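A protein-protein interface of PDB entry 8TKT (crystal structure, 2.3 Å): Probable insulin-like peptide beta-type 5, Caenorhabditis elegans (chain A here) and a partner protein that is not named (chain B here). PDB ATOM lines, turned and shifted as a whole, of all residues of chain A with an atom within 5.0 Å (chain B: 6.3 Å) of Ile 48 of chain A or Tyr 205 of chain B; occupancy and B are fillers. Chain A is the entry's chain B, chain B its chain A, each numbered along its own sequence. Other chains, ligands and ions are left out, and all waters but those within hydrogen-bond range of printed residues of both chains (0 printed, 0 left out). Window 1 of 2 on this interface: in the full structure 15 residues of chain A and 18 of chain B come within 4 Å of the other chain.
Of chain B, only Tyr 205 (3.6 Å) comes within 4 Å of Ile 48 of chain A. Of chain A, only Cys 38, Asn 41, Gln 42, Cys 43 and Ile 48 come within 4 Å of Tyr 205 of chain B. Printed residues of chain B within 4 Å of Ser 44 of chain A: Thr 207 and Ala 208. Of the printed residues of chain A, Phe 203 of chain B touches Cys 10. Printed residues of chain B within 4 Å of Leu 17 of chain A: Phe 132 (3.5 Å). Printed residues of chain A within 4 Å of Trp 181 of chain B: Cys 38 (3.4 Å), Asn 41 (3.9 Å) and Gln 42 (3.4 Å). Arg 49 of chain A touches none of the printed residues of chain B. The nearest printed residue of chain B that does not touch Asp 45 of chain A is Ala 208 of chain B (4.4 Å).
Cys 10 of chain A touches Phe 203 of chain B. CE2 of Phe 132 of chain B touches CD2 of Leu 14 of chain A, at 3.4 Å. Phe 132 of chain B touches Leu 17 of chain A. Trp 181 of chain B touches Cys 38 of chain A (CH2 to O, 3.4 Å). CZ2 of Trp 181 of chain B touches C of Asn 41 of chain A, at 3.9 Å. Gln 42 of chain A touches Trp 181 of chain B (NE2 to CB, 3.4 Å). NE2 of Gln 42 of chain A touches C of Thr 207 of chain B, at 3.8 Å. CG of Gln 42 of chain A touches N of Ala 208 of chain B, at 3.5 Å. Ser 44 of chain A touches Thr 207 of chain B (C to CB, 3.99 Å). Ala 208 of chain B touches Ser 44 of chain A (CB to N, 3.7 Å).
O of Pro 206 of chain B is in hydrogen-bond range of NE2 of Gln 42 of chain A. N of Ala 208 of chain B lies within hydrogen-bond range of O of Cys 43 of chain A (2.7 Å). OH of Tyr 205 of chain B is in hydrogen-bond range of O of Cys 38 of chain A, 2.6 Å away. The side-chain hydroxyl (OH) of Tyr 205 of chain B is in hydrogen-bond range of the backbone NH (N) of Cys 43 of chain A, 2.9 Å away.
Of the 15 printed residues of chain B, 7 touch a printed residue of chain A. Printed residues of chain B that touch a printed residue of chain A: Phe 132, Trp 181, Phe 203, Tyr 205, Pro 206, Thr 207 and Ala 208. Among the printed residues, 19 pairs touch across the chains. Among the printed residues, no Asp or Glu carboxylate lies within 4 Å of a Lys or Arg side-chain nitrogen of the other chain.
OD1 of Asp 45 of chain A is in salt-bridge range of NE of Arg 49 of chain A. The backbone NH of Thr 207 of chain B lies within hydrogen-bond range of the backbone carbonyl oxygen of Glu 133 of chain B (2.7 Å). The backbone carbonyl oxygen (O) of Arg 131 of chain B is in hydrogen-bond range of the backbone NH (N) of Tyr 205 of chain B, 2.9 Å away. O of Phe 203 of chain B lies within hydrogen-bond range of N of Arg 131 of chain B, 2.9 Å away. The side-chain sulfur of Cys 10 of chain A is disulfide-bonded to the side-chain sulfur of Cys 39 of chain A (2.0 Å). N of Glu 133 of chain B lies within hydrogen-bond range of O of Tyr 205 of chain B.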
ATOM      1  N   CYS A  10      18.045 -15.281  24.791  1.00  0.00           N
ATOM      2  CA  CYS A  10      16.947 -15.226  23.833  1.00  0.00           C
ATOM      3  C   CYS A  10      16.282 -13.855  23.841  1.00  0.00           C
ATOM      4  O   CYS A  10      16.169 -13.194  22.803  1.00  0.00           O
ATOM      5  CB  CYS A  10      15.936 -16.330  24.150  1.00  0.00           C
ATOM      6  SG  CYS A  10      14.512 -16.377  23.040  1.00  0.00           S
ATOM      7  N   LEU A  14      16.141 -11.131  20.781  1.00  0.00           N
ATOM      8  CA  LEU A  14      14.834 -10.784  20.230  1.00  0.00           C
ATOM      9  C   LEU A  14      14.564  -9.290  20.352  1.00  0.00           C
ATOM     10  O   LEU A  14      14.115  -8.648  19.395  1.00  0.00           O
ATOM     11  CB  LEU A  14      13.742 -11.583  20.939  1.00  0.00           C
ATOM     12  CG  LEU A  14      13.225 -12.831  20.229  1.00  0.00           C
ATOM     13  CD1 LEU A  14      12.118 -13.458  21.040  1.00  0.00           C
ATOM     14  CD2 LEU A  14      12.713 -12.460  18.857  1.00  0.00           C
ATOM     15  N   LEU A  17      16.442  -7.355  17.707  1.00  0.00           N
ATOM     16  CA  LEU A  17      15.841  -7.397  16.377  1.00  0.00           C
ATOM     17  C   LEU A  17      14.589  -6.536  16.313  1.00  0.00           C
ATOM     18  O   LEU A  17      14.347  -5.849  15.314  1.00  0.00           O
ATOM     19  CB  LEU A  17      15.504  -8.835  15.984  1.00  0.00           C
ATOM     20  CG  LEU A  17      14.795  -8.965  14.631  1.00  0.00           C
ATOM     21  CD1 LEU A  17      15.792  -8.868  13.486  1.00  0.00           C
ATOM     22  CD2 LEU A  17      13.970 -10.241  14.534  1.00  0.00           C
ATOM     23  N   VAL A  18      13.780  -6.560  17.373  1.00  0.00           N
ATOM     24  CA  VAL A  18      12.521  -5.822  17.374  1.00  0.00           C
ATOM     25  C   VAL A  18      12.782  -4.321  17.342  1.00  0.00           C
ATOM     26  O   VAL A  18      12.172  -3.584  16.557  1.00  0.00           O
ATOM     27  CB  VAL A  18      11.670  -6.228  18.592  1.00  0.00           C
ATOM     28  CG1 VAL A  18      10.613  -5.178  18.885  1.00  0.00           C
ATOM     29  CG2 VAL A  18      11.026  -7.587  18.363  1.00  0.00           C
ATOM     30  N   CYS A  38       7.824 -14.748  23.134  1.00  0.00           N
ATOM     31  CA  CYS A  38       8.405 -15.523  22.048  1.00  0.00           C
ATOM     32  C   CYS A  38       9.613 -16.351  22.466  1.00  0.00           C
ATOM     33  O   CYS A  38      10.087 -17.164  21.665  1.00  0.00           O
ATOM     34  CB  CYS A  38       8.775 -14.593  20.894  1.00  0.00           C
ATOM     35  SG  CYS A  38       7.328 -13.823  20.159  1.00  0.00           S
ATOM     36  N   CYS A  39      10.120 -16.176  23.684  1.00  0.00           N
ATOM     37  CA  CYS A  39      11.167 -17.043  24.200  1.00  0.00           C
ATOM     38  C   CYS A  39      10.623 -18.167  25.067  1.00  0.00           C
ATOM     39  O   CYS A  39      11.360 -19.113  25.366  1.00  0.00           O
ATOM     40  CB  CYS A  39      12.190 -16.224  24.994  1.00  0.00           C
ATOM     41  SG  CYS A  39      13.181 -15.138  23.945  1.00  0.00           S
ATOM     42  N   ASN A  41       7.384 -19.514  24.137  1.00  0.00           N
ATOM     43  CA  ASN A  41       6.658 -20.258  23.121  1.00  0.00           C
ATOM     44  C   ASN A  41       7.123 -19.807  21.744  1.00  0.00           C
ATOM     45  O   ASN A  41       7.571 -18.671  21.567  1.00  0.00           O
ATOM     46  CB  ASN A  41       5.148 -20.044  23.261  1.00  0.00           C
ATOM     47  CG  ASN A  41       4.622 -20.494  24.609  1.00  0.00           C
ATOM     48  OD1 ASN A  41       4.349 -21.675  24.821  1.00  0.00           O
ATOM     49  ND2 ASN A  41       4.486 -19.550  25.534  1.00  0.00           N
ATOM     50  N   GLN A  42       7.020 -20.706  20.767  1.00  0.00           N
ATOM     51  CA  GLN A  42       7.496 -20.399  19.423  1.00  0.00           C
ATOM     52  C   GLN A  42       6.559 -19.402  18.753  1.00  0.00           C
ATOM     53  O   GLN A  42       5.353 -19.650  18.647  1.00  0.00           O
ATOM     54  CB  GLN A  42       7.612 -21.667  18.581  1.00  0.00           C
ATOM     55  CG  GLN A  42       8.162 -21.404  17.182  1.00  0.00           C
ATOM     56  CD  GLN A  42       8.430 -22.673  16.399  1.00  0.00           C
ATOM     57  OE1 GLN A  42       7.516 -23.446  16.117  1.00  0.00           O
ATOM     58  NE2 GLN A  42       9.692 -22.894  16.044  1.00  0.00           N
ATOM     59  N   CYS A  43       7.110 -18.280  18.305  1.00  0.00           N
ATOM     60  CA  CYS A  43       6.370 -17.273  17.561  1.00  0.00           C
ATOM     61  C   CYS A  43       6.668 -17.386  16.071  1.00  0.00           C
ATOM     62  O   CYS A  43       7.690 -17.937  15.654  1.00  0.00           O
ATOM     63  CB  CYS A  43       6.720 -15.861  18.037  1.00  0.00           C
ATOM     64  SG  CYS A  43       6.161 -15.417  19.688  1.00  0.00           S
ATOM     65  N   SER A  44       5.753 -16.851  15.268  1.00  0.00           N
ATOM     66  CA  SER A  44       5.988 -16.773  13.838  1.00  0.00           C
ATOM     67  C   SER A  44       6.924 -15.609  13.529  1.00  0.00           C
ATOM     68  O   SER A  44       7.169 -14.734  14.365  1.00  0.00           O
ATOM     69  CB  SER A  44       4.670 -16.613  13.087  1.00  0.00           C
ATOM     70  OG  SER A  44       4.068 -15.365  13.378  1.00  0.00           O
ATOM     71  N   ASP A  45       7.454 -15.600  12.306  1.00  0.00           N
ATOM     72  CA  ASP A  45       8.318 -14.499  11.900  1.00  0.00           C
ATOM     73  C   ASP A  45       7.544 -13.192  11.795  1.00  0.00           C
ATOM     74  O   ASP A  45       8.029 -12.141  12.230  1.00  0.00           O
ATOM     75  CB  ASP A  45       8.997 -14.818  10.571  1.00  0.00           C
ATOM     76  CG  ASP A  45       9.569 -13.585   9.902  1.00  0.00           C
ATOM     77  OD1 ASP A  45      10.436 -12.924  10.513  1.00  0.00           O
ATOM     78  OD2 ASP A  45       9.154 -13.276   8.767  1.00  0.00           O
ATOM     79  N   ASP A  46       6.343 -13.236  11.209  1.00  0.00           N
ATOM     80  CA  ASP A  46       5.583 -12.009  10.995  1.00  0.00           C
ATOM     81  C   ASP A  46       5.236 -11.341  12.318  1.00  0.00           C
ATOM     82  O   ASP A  46       5.338 -10.116  12.448  1.00  0.00           O
ATOM     83  CB  ASP A  46       4.319 -12.296  10.184  1.00  0.00           C
ATOM     84  CG  ASP A  46       3.501 -11.042   9.924  1.00  0.00           C
ATOM     85  OD1 ASP A  46       3.818 -10.317   8.955  1.00  0.00           O
ATOM     86  OD2 ASP A  46       2.548 -10.775  10.686  1.00  0.00           O
ATOM     87  N   TYR A  47       4.810 -12.131  13.307  1.00  0.00           N
ATOM     88  CA  TYR A  47       4.515 -11.576  14.623  1.00  0.00           C
ATOM     89  C   TYR A  47       5.737 -10.872  15.198  1.00  0.00           C
ATOM     90  O   TYR A  47       5.646  -9.738  15.674  1.00  0.00           O
ATOM     91  CB  TYR A  47       4.029 -12.676  15.567  1.00  0.00           C
ATOM     92  CG  TYR A  47       3.685 -12.177  16.955  1.00  0.00           C
ATOM     93  CD1 TYR A  47       2.491 -11.509  17.200  1.00  0.00           C
ATOM     94  CD2 TYR A  47       4.556 -12.371  18.022  1.00  0.00           C
ATOM     95  CE1 TYR A  47       2.172 -11.049  18.466  1.00  0.00           C
ATOM     96  CE2 TYR A  47       4.247 -11.914  19.292  1.00  0.00           C
ATOM     97  CZ  TYR A  47       3.053 -11.253  19.508  1.00  0.00           C
ATOM     98  OH  TYR A  47       2.741 -10.796  20.768  1.00  0.00           O
ATOM     99  N   ILE A  48       6.895 -11.534  15.153  1.00  0.00           N
ATOM    100  CA  ILE A  48       8.102 -10.968  15.755  1.00  0.00           C
ATOM    101  C   ILE A  48       8.438  -9.628  15.108  1.00  0.00           C
ATOM    102  O   ILE A  48       8.742  -8.645  15.795  1.00  0.00           O
ATOM    103  CB  ILE A  48       9.274 -11.959  15.639  1.00  0.00           C
ATOM    104  CG1 ILE A  48       9.020 -13.198  16.502  1.00  0.00           C
ATOM    105  CG2 ILE A  48      10.585 -11.291  16.026  1.00  0.00           C
ATOM    106  CD1 ILE A  48      10.065 -14.277  16.331  1.00  0.00           C
ATOM    107  N   ARG A  49       8.383  -9.570  13.778  1.00  0.00           N
ATOM    108  CA  ARG A  49       8.803  -8.384  13.039  1.00  0.00           C
ATOM    109  C   ARG A  49       7.777  -7.257  13.040  1.00  0.00           C
ATOM    110  O   ARG A  49       8.115  -6.143  12.628  1.00  0.00           O
ATOM    111  CB  ARG A  49       9.119  -8.761  11.591  1.00  0.00           C
ATOM    112  CG  ARG A  49      10.462  -9.439  11.384  1.00  0.00           C
ATOM    113  CD  ARG A  49      10.793  -9.619   9.901  1.00  0.00           C
ATOM    114  NE  ARG A  49       9.805 -10.428   9.195  1.00  0.00           N
ATOM    115  CZ  ARG A  49       8.757  -9.945   8.539  1.00  0.00           C
ATOM    116  NH1 ARG A  49       8.541  -8.643   8.439  1.00  0.00           N
ATOM    117  NH2 ARG A  49       7.903 -10.790   7.967  1.00  0.00           N
ATOM    118  N   SER A  50       6.538  -7.501  13.471  1.00  0.00           N
ATOM    119  CA  SER A  50       5.512  -6.468  13.403  1.00  0.00           C
ATOM    120  C   SER A  50       4.707  -6.255  14.679  1.00  0.00           C
ATOM    121  O   SER A  50       3.955  -5.277  14.738  1.00  0.00           O
ATOM    122  CB  SER A  50       4.532  -6.761  12.256  1.00  0.00           C
ATOM    123  OG  SER A  50       3.838  -7.976  12.477  1.00  0.00           O
ATOM    124  N   ALA A  51       4.822  -7.125  15.689  1.00  0.00           N
ATOM    125  CA  ALA A  51       3.950  -7.014  16.858  1.00  0.00           C
ATOM    126  C   ALA A  51       4.130  -5.692  17.591  1.00  0.00           C
ATOM    127  O   ALA A  51       3.177  -5.182  18.191  1.00  0.00           O
ATOM    128  CB  ALA A  51       4.190  -8.176  17.823  1.00  0.00           C
ATOM    129  N   ARG B 131      20.029 -15.241  14.167  1.00  0.00           N
ATOM    130  CA  ARG B 131      19.497 -15.746  12.910  1.00  0.00           C
ATOM    131  C   ARG B 131      18.089 -16.258  13.150  1.00  0.00           C
ATOM    132  O   ARG B 131      17.873 -17.096  14.030  1.00  0.00           O
ATOM    133  CB  ARG B 131      20.369 -16.867  12.329  1.00  0.00           C
ATOM    134  CG  ARG B 131      19.696 -17.666  11.208  1.00  0.00           C
ATOM    135  CD  ARG B 131      19.504 -16.832   9.942  1.00  0.00           C
ATOM    136  NE  ARG B 131      18.723 -17.532   8.926  1.00  0.00           N
ATOM    137  CZ  ARG B 131      19.239 -18.288   7.963  1.00  0.00           C
ATOM    138  NH1 ARG B 131      18.467 -18.971   7.132  1.00  0.00           N
ATOM    139  NH2 ARG B 131      20.560 -18.374   7.841  1.00  0.00           N
ATOM    140  N   PHE B 132      17.138 -15.747  12.377  1.00  0.00           N
ATOM    141  CA  PHE B 132      15.756 -16.201  12.420  1.00  0.00           C
ATOM    142  C   PHE B 132      15.453 -16.950  11.132  1.00  0.00           C
ATOM    143  O   PHE B 132      15.788 -16.477  10.041  1.00  0.00           O
ATOM    144  CB  PHE B 132      14.795 -15.025  12.615  1.00  0.00           C
ATOM    145  CG  PHE B 132      14.954 -14.339  13.945  1.00  0.00           C
ATOM    146  CD1 PHE B 132      16.004 -13.460  14.166  1.00  0.00           C
ATOM    147  CD2 PHE B 132      14.077 -14.600  14.984  1.00  0.00           C
ATOM    148  CE1 PHE B 132      16.166 -12.841  15.391  1.00  0.00           C
ATOM    149  CE2 PHE B 132      14.236 -13.987  16.211  1.00  0.00           C
ATOM    150  CZ  PHE B 132      15.280 -13.103  16.416  1.00  0.00           C
ATOM    151  N   GLU B 133      14.820 -18.110  11.261  1.00  0.00           N
ATOM    152  CA  GLU B 133      14.529 -18.930  10.097  1.00  0.00           C
ATOM    153  C   GLU B 133      13.335 -19.814  10.420  1.00  0.00           C
ATOM    154  O   GLU B 133      13.065 -20.107  11.587  1.00  0.00           O
ATOM    155  CB  GLU B 133      15.745 -19.771   9.696  1.00  0.00           C
ATOM    156  CG  GLU B 133      15.624 -20.435   8.339  1.00  0.00           C
ATOM    157  CD  GLU B 133      15.084 -19.493   7.284  1.00  0.00           C
ATOM    158  OE1 GLU B 133      15.854 -18.638   6.802  1.00  0.00           O
ATOM    159  OE2 GLU B 133      13.892 -19.611   6.935  1.00  0.00           O
ATOM    160  N   MET B 134      12.618 -20.223   9.379  1.00  0.00           N
ATOM    161  CA  MET B 134      11.393 -20.987   9.555  1.00  0.00           C
ATOM    162  C   MET B 134      11.699 -22.452   9.836  1.00  0.00           C
ATOM    163  O   MET B 134      12.628 -23.028   9.263  1.00  0.00           O
ATOM    164  CB  MET B 134      10.519 -20.874   8.308  1.00  0.00           C
ATOM    165  CG  MET B 134       9.100 -21.373   8.487  1.00  0.00           C
ATOM    166  SD  MET B 134       8.145 -21.134   6.979  1.00  0.00           S
ATOM    167  CE  MET B 134       8.233 -19.353   6.810  1.00  0.00           C
ATOM    168  N   ILE B 179      15.395 -27.383  10.710  1.00  0.00           N
ATOM    169  CA  ILE B 179      15.432 -26.851  12.067  1.00  0.00           C
ATOM    170  C   ILE B 179      14.071 -27.005  12.736  1.00  0.00           C
ATOM    171  O   ILE B 179      13.018 -27.003  12.084  1.00  0.00           O
ATOM    172  CB  ILE B 179      15.887 -25.379  12.073  1.00  0.00           C
ATOM    173  CG1 ILE B 179      14.833 -24.479  11.422  1.00  0.00           C
ATOM    174  CG2 ILE B 179      17.227 -25.234  11.366  1.00  0.00           C
ATOM    175  CD1 ILE B 179      15.253 -23.027  11.323  1.00  0.00           C
ATOM    176  N   TRP B 181      11.939 -26.176  16.785  1.00  0.00           N
ATOM    177  CA  TRP B 181      11.931 -25.245  17.910  1.00  0.00           C
ATOM    178  C   TRP B 181      12.920 -25.641  19.003  1.00  0.00           C
ATOM    179  O   TRP B 181      13.404 -24.774  19.740  1.00  0.00           O
ATOM    180  CB  TRP B 181      10.516 -25.128  18.480  1.00  0.00           C
ATOM    181  CG  TRP B 181      10.436 -24.301  19.729  1.00  0.00           C
ATOM    182  CD1 TRP B 181      10.083 -24.729  20.974  1.00  0.00           C
ATOM    183  CD2 TRP B 181      10.743 -22.906  19.856  1.00  0.00           C
ATOM    184  NE1 TRP B 181      10.134 -23.684  21.866  1.00  0.00           N
ATOM    185  CE2 TRP B 181      10.539 -22.555  21.205  1.00  0.00           C
ATOM    186  CE3 TRP B 181      11.165 -21.919  18.958  1.00  0.00           C
ATOM    187  CZ2 TRP B 181      10.742 -21.259  21.678  1.00  0.00           C
ATOM    188  CZ3 TRP B 181      11.366 -20.633  19.430  1.00  0.00           C
ATOM    189  CH2 TRP B 181      11.154 -20.316  20.777  1.00  0.00           C
ATOM    190  N   ASP B 183      15.882 -26.538  18.495  1.00  0.00           N
ATOM    191  CA  ASP B 183      17.184 -26.012  18.103  1.00  0.00           C
ATOM    192  C   ASP B 183      17.391 -24.575  18.551  1.00  0.00           C
ATOM    193  O   ASP B 183      18.509 -24.061  18.434  1.00  0.00           O
ATOM    194  CB  ASP B 183      17.360 -26.097  16.587  1.00  0.00           C
ATOM    195  CG  ASP B 183      17.349 -27.517  16.081  1.00  0.00           C
ATOM    196  OD1 ASP B 183      18.063 -28.358  16.667  1.00  0.00           O
ATOM    197  OD2 ASP B 183      16.624 -27.790  15.102  1.00  0.00           O
ATOM    198  N   MET B 184      16.341 -23.919  19.039  1.00  0.00           N
ATOM    199  CA  MET B 184      16.455 -22.539  19.485  1.00  0.00           C
ATOM    200  C   MET B 184      17.451 -22.442  20.631  1.00  0.00           C
ATOM    201  O   MET B 184      17.463 -23.278  21.536  1.00  0.00           O
ATOM    202  CB  MET B 184      15.086 -22.024  19.933  1.00  0.00           C
ATOM    203  CG  MET B 184      15.018 -20.536  20.237  1.00  0.00           C
ATOM    204  SD  MET B 184      15.508 -20.174  21.936  1.00  0.00           S
ATOM    205  CE  MET B 184      14.176 -20.963  22.838  1.00  0.00           C
ATOM    206  N   GLY B 185      18.288 -21.416  20.590  1.00  0.00           N
ATOM    207  CA  GLY B 185      19.171 -21.124  21.692  1.00  0.00           C
ATOM    208  C   GLY B 185      20.536 -20.688  21.210  1.00  0.00           C
ATOM    209  O   GLY B 185      20.742 -20.378  20.038  1.00  0.00           O
ATOM    210  N   PHE B 203      23.190 -17.044  18.002  1.00  0.00           N
ATOM    211  CA  PHE B 203      21.846 -17.366  18.453  1.00  0.00           C
ATOM    212  C   PHE B 203      20.968 -17.727  17.266  1.00  0.00           C
ATOM    213  O   PHE B 203      21.027 -17.079  16.218  1.00  0.00           O
ATOM    214  CB  PHE B 203      21.227 -16.199  19.232  1.00  0.00           C
ATOM    215  CG  PHE B 203      19.812 -16.448  19.670  1.00  0.00           C
ATOM    216  CD1 PHE B 203      19.545 -17.270  20.753  1.00  0.00           C
ATOM    217  CD2 PHE B 203      18.750 -15.853  19.006  1.00  0.00           C
ATOM    218  CE1 PHE B 203      18.246 -17.504  21.160  1.00  0.00           C
ATOM    219  CE2 PHE B 203      17.447 -16.081  19.410  1.00  0.00           C
ATOM    220  CZ  PHE B 203      17.194 -16.908  20.488  1.00  0.00           C
ATOM    221  N   LEU B 204      20.150 -18.762  17.447  1.00  0.00           N
ATOM    222  CA  LEU B 204      19.274 -19.278  16.406  1.00  0.00           C
ATOM    223  C   LEU B 204      17.848 -19.314  16.930  1.00  0.00           C
ATOM    224  O   LEU B 204      17.603 -19.825  18.027  1.00  0.00           O
ATOM    225  CB  LEU B 204      19.698 -20.680  15.959  1.00  0.00           C
ATOM    226  CG  LEU B 204      18.752 -21.327  14.946  1.00  0.00           C
ATOM    227  CD1 LEU B 204      18.851 -20.623  13.605  1.00  0.00           C
ATOM    228  CD2 LEU B 204      19.036 -22.811  14.800  1.00  0.00           C
ATOM    229  N   TYR B 205      16.914 -18.780  16.147  1.00  0.00           N
ATOM    230  CA  TYR B 205      15.495 -18.797  16.498  1.00  0.00           C
ATOM    231  C   TYR B 205      14.688 -19.377  15.344  1.00  0.00           C
ATOM    232  O   TYR B 205      14.480 -18.701  14.324  1.00  0.00           O
ATOM    233  CB  TYR B 205      14.991 -17.402  16.849  1.00  0.00           C
ATOM    234  CG  TYR B 205      13.605 -17.394  17.457  1.00  0.00           C
ATOM    235  CD1 TYR B 205      12.474 -17.547  16.662  1.00  0.00           C
ATOM    236  CD2 TYR B 205      13.427 -17.233  18.822  1.00  0.00           C
ATOM    237  CE1 TYR B 205      11.210 -17.546  17.211  1.00  0.00           C
ATOM    238  CE2 TYR B 205      12.165 -17.228  19.380  1.00  0.00           C
ATOM    239  CZ  TYR B 205      11.059 -17.384  18.570  1.00  0.00           C
ATOM    240  OH  TYR B 205       9.798 -17.382  19.118  1.00  0.00           O
ATOM    241  N   PRO B 206      14.217 -20.623  15.466  1.00  0.00           N
ATOM    242  CA  PRO B 206      13.287 -21.173  14.469  1.00  0.00           C
ATOM    243  C   PRO B 206      11.903 -20.581  14.667  1.00  0.00           C
ATOM    244  O   PRO B 206      11.305 -20.719  15.739  1.00  0.00           O
ATOM    245  CB  PRO B 206      13.306 -22.681  14.761  1.00  0.00           C
ATOM    246  CG  PRO B 206      14.494 -22.902  15.662  1.00  0.00           C
ATOM    247  CD  PRO B 206      14.639 -21.637  16.440  1.00  0.00           C
ATOM    248  N   THR B 207      11.389 -19.913  13.639  1.00  0.00           N
ATOM    249  CA  THR B 207      10.088 -19.269  13.733  1.00  0.00           C
ATOM    250  C   THR B 207       8.984 -20.257  13.380  1.00  0.00           C
ATOM    251  O   THR B 207       9.191 -21.211  12.625  1.00  0.00           O
ATOM    252  CB  THR B 207      10.002 -18.051  12.811  1.00  0.00           C
ATOM    253  OG1 THR B 207      10.291 -18.445  11.464  1.00  0.00           O
ATOM    254  CG2 THR B 207      10.990 -16.979  13.244  1.00  0.00           C
ATOM    255  N   ALA B 208       7.803 -20.020  13.949  1.00  0.00           N
ATOM    256  CA  ALA B 208       6.654 -20.878  13.693  1.00  0.00           C
ATOM    257  C   ALA B 208       6.273 -20.848  12.216  1.00  0.00           C
ATOM    258  O   ALA B 208       6.380 -19.822  11.539  1.00  0.00           O
ATOM    259  CB  ALA B 208       5.468 -20.450  14.557  1.00  0.00           C
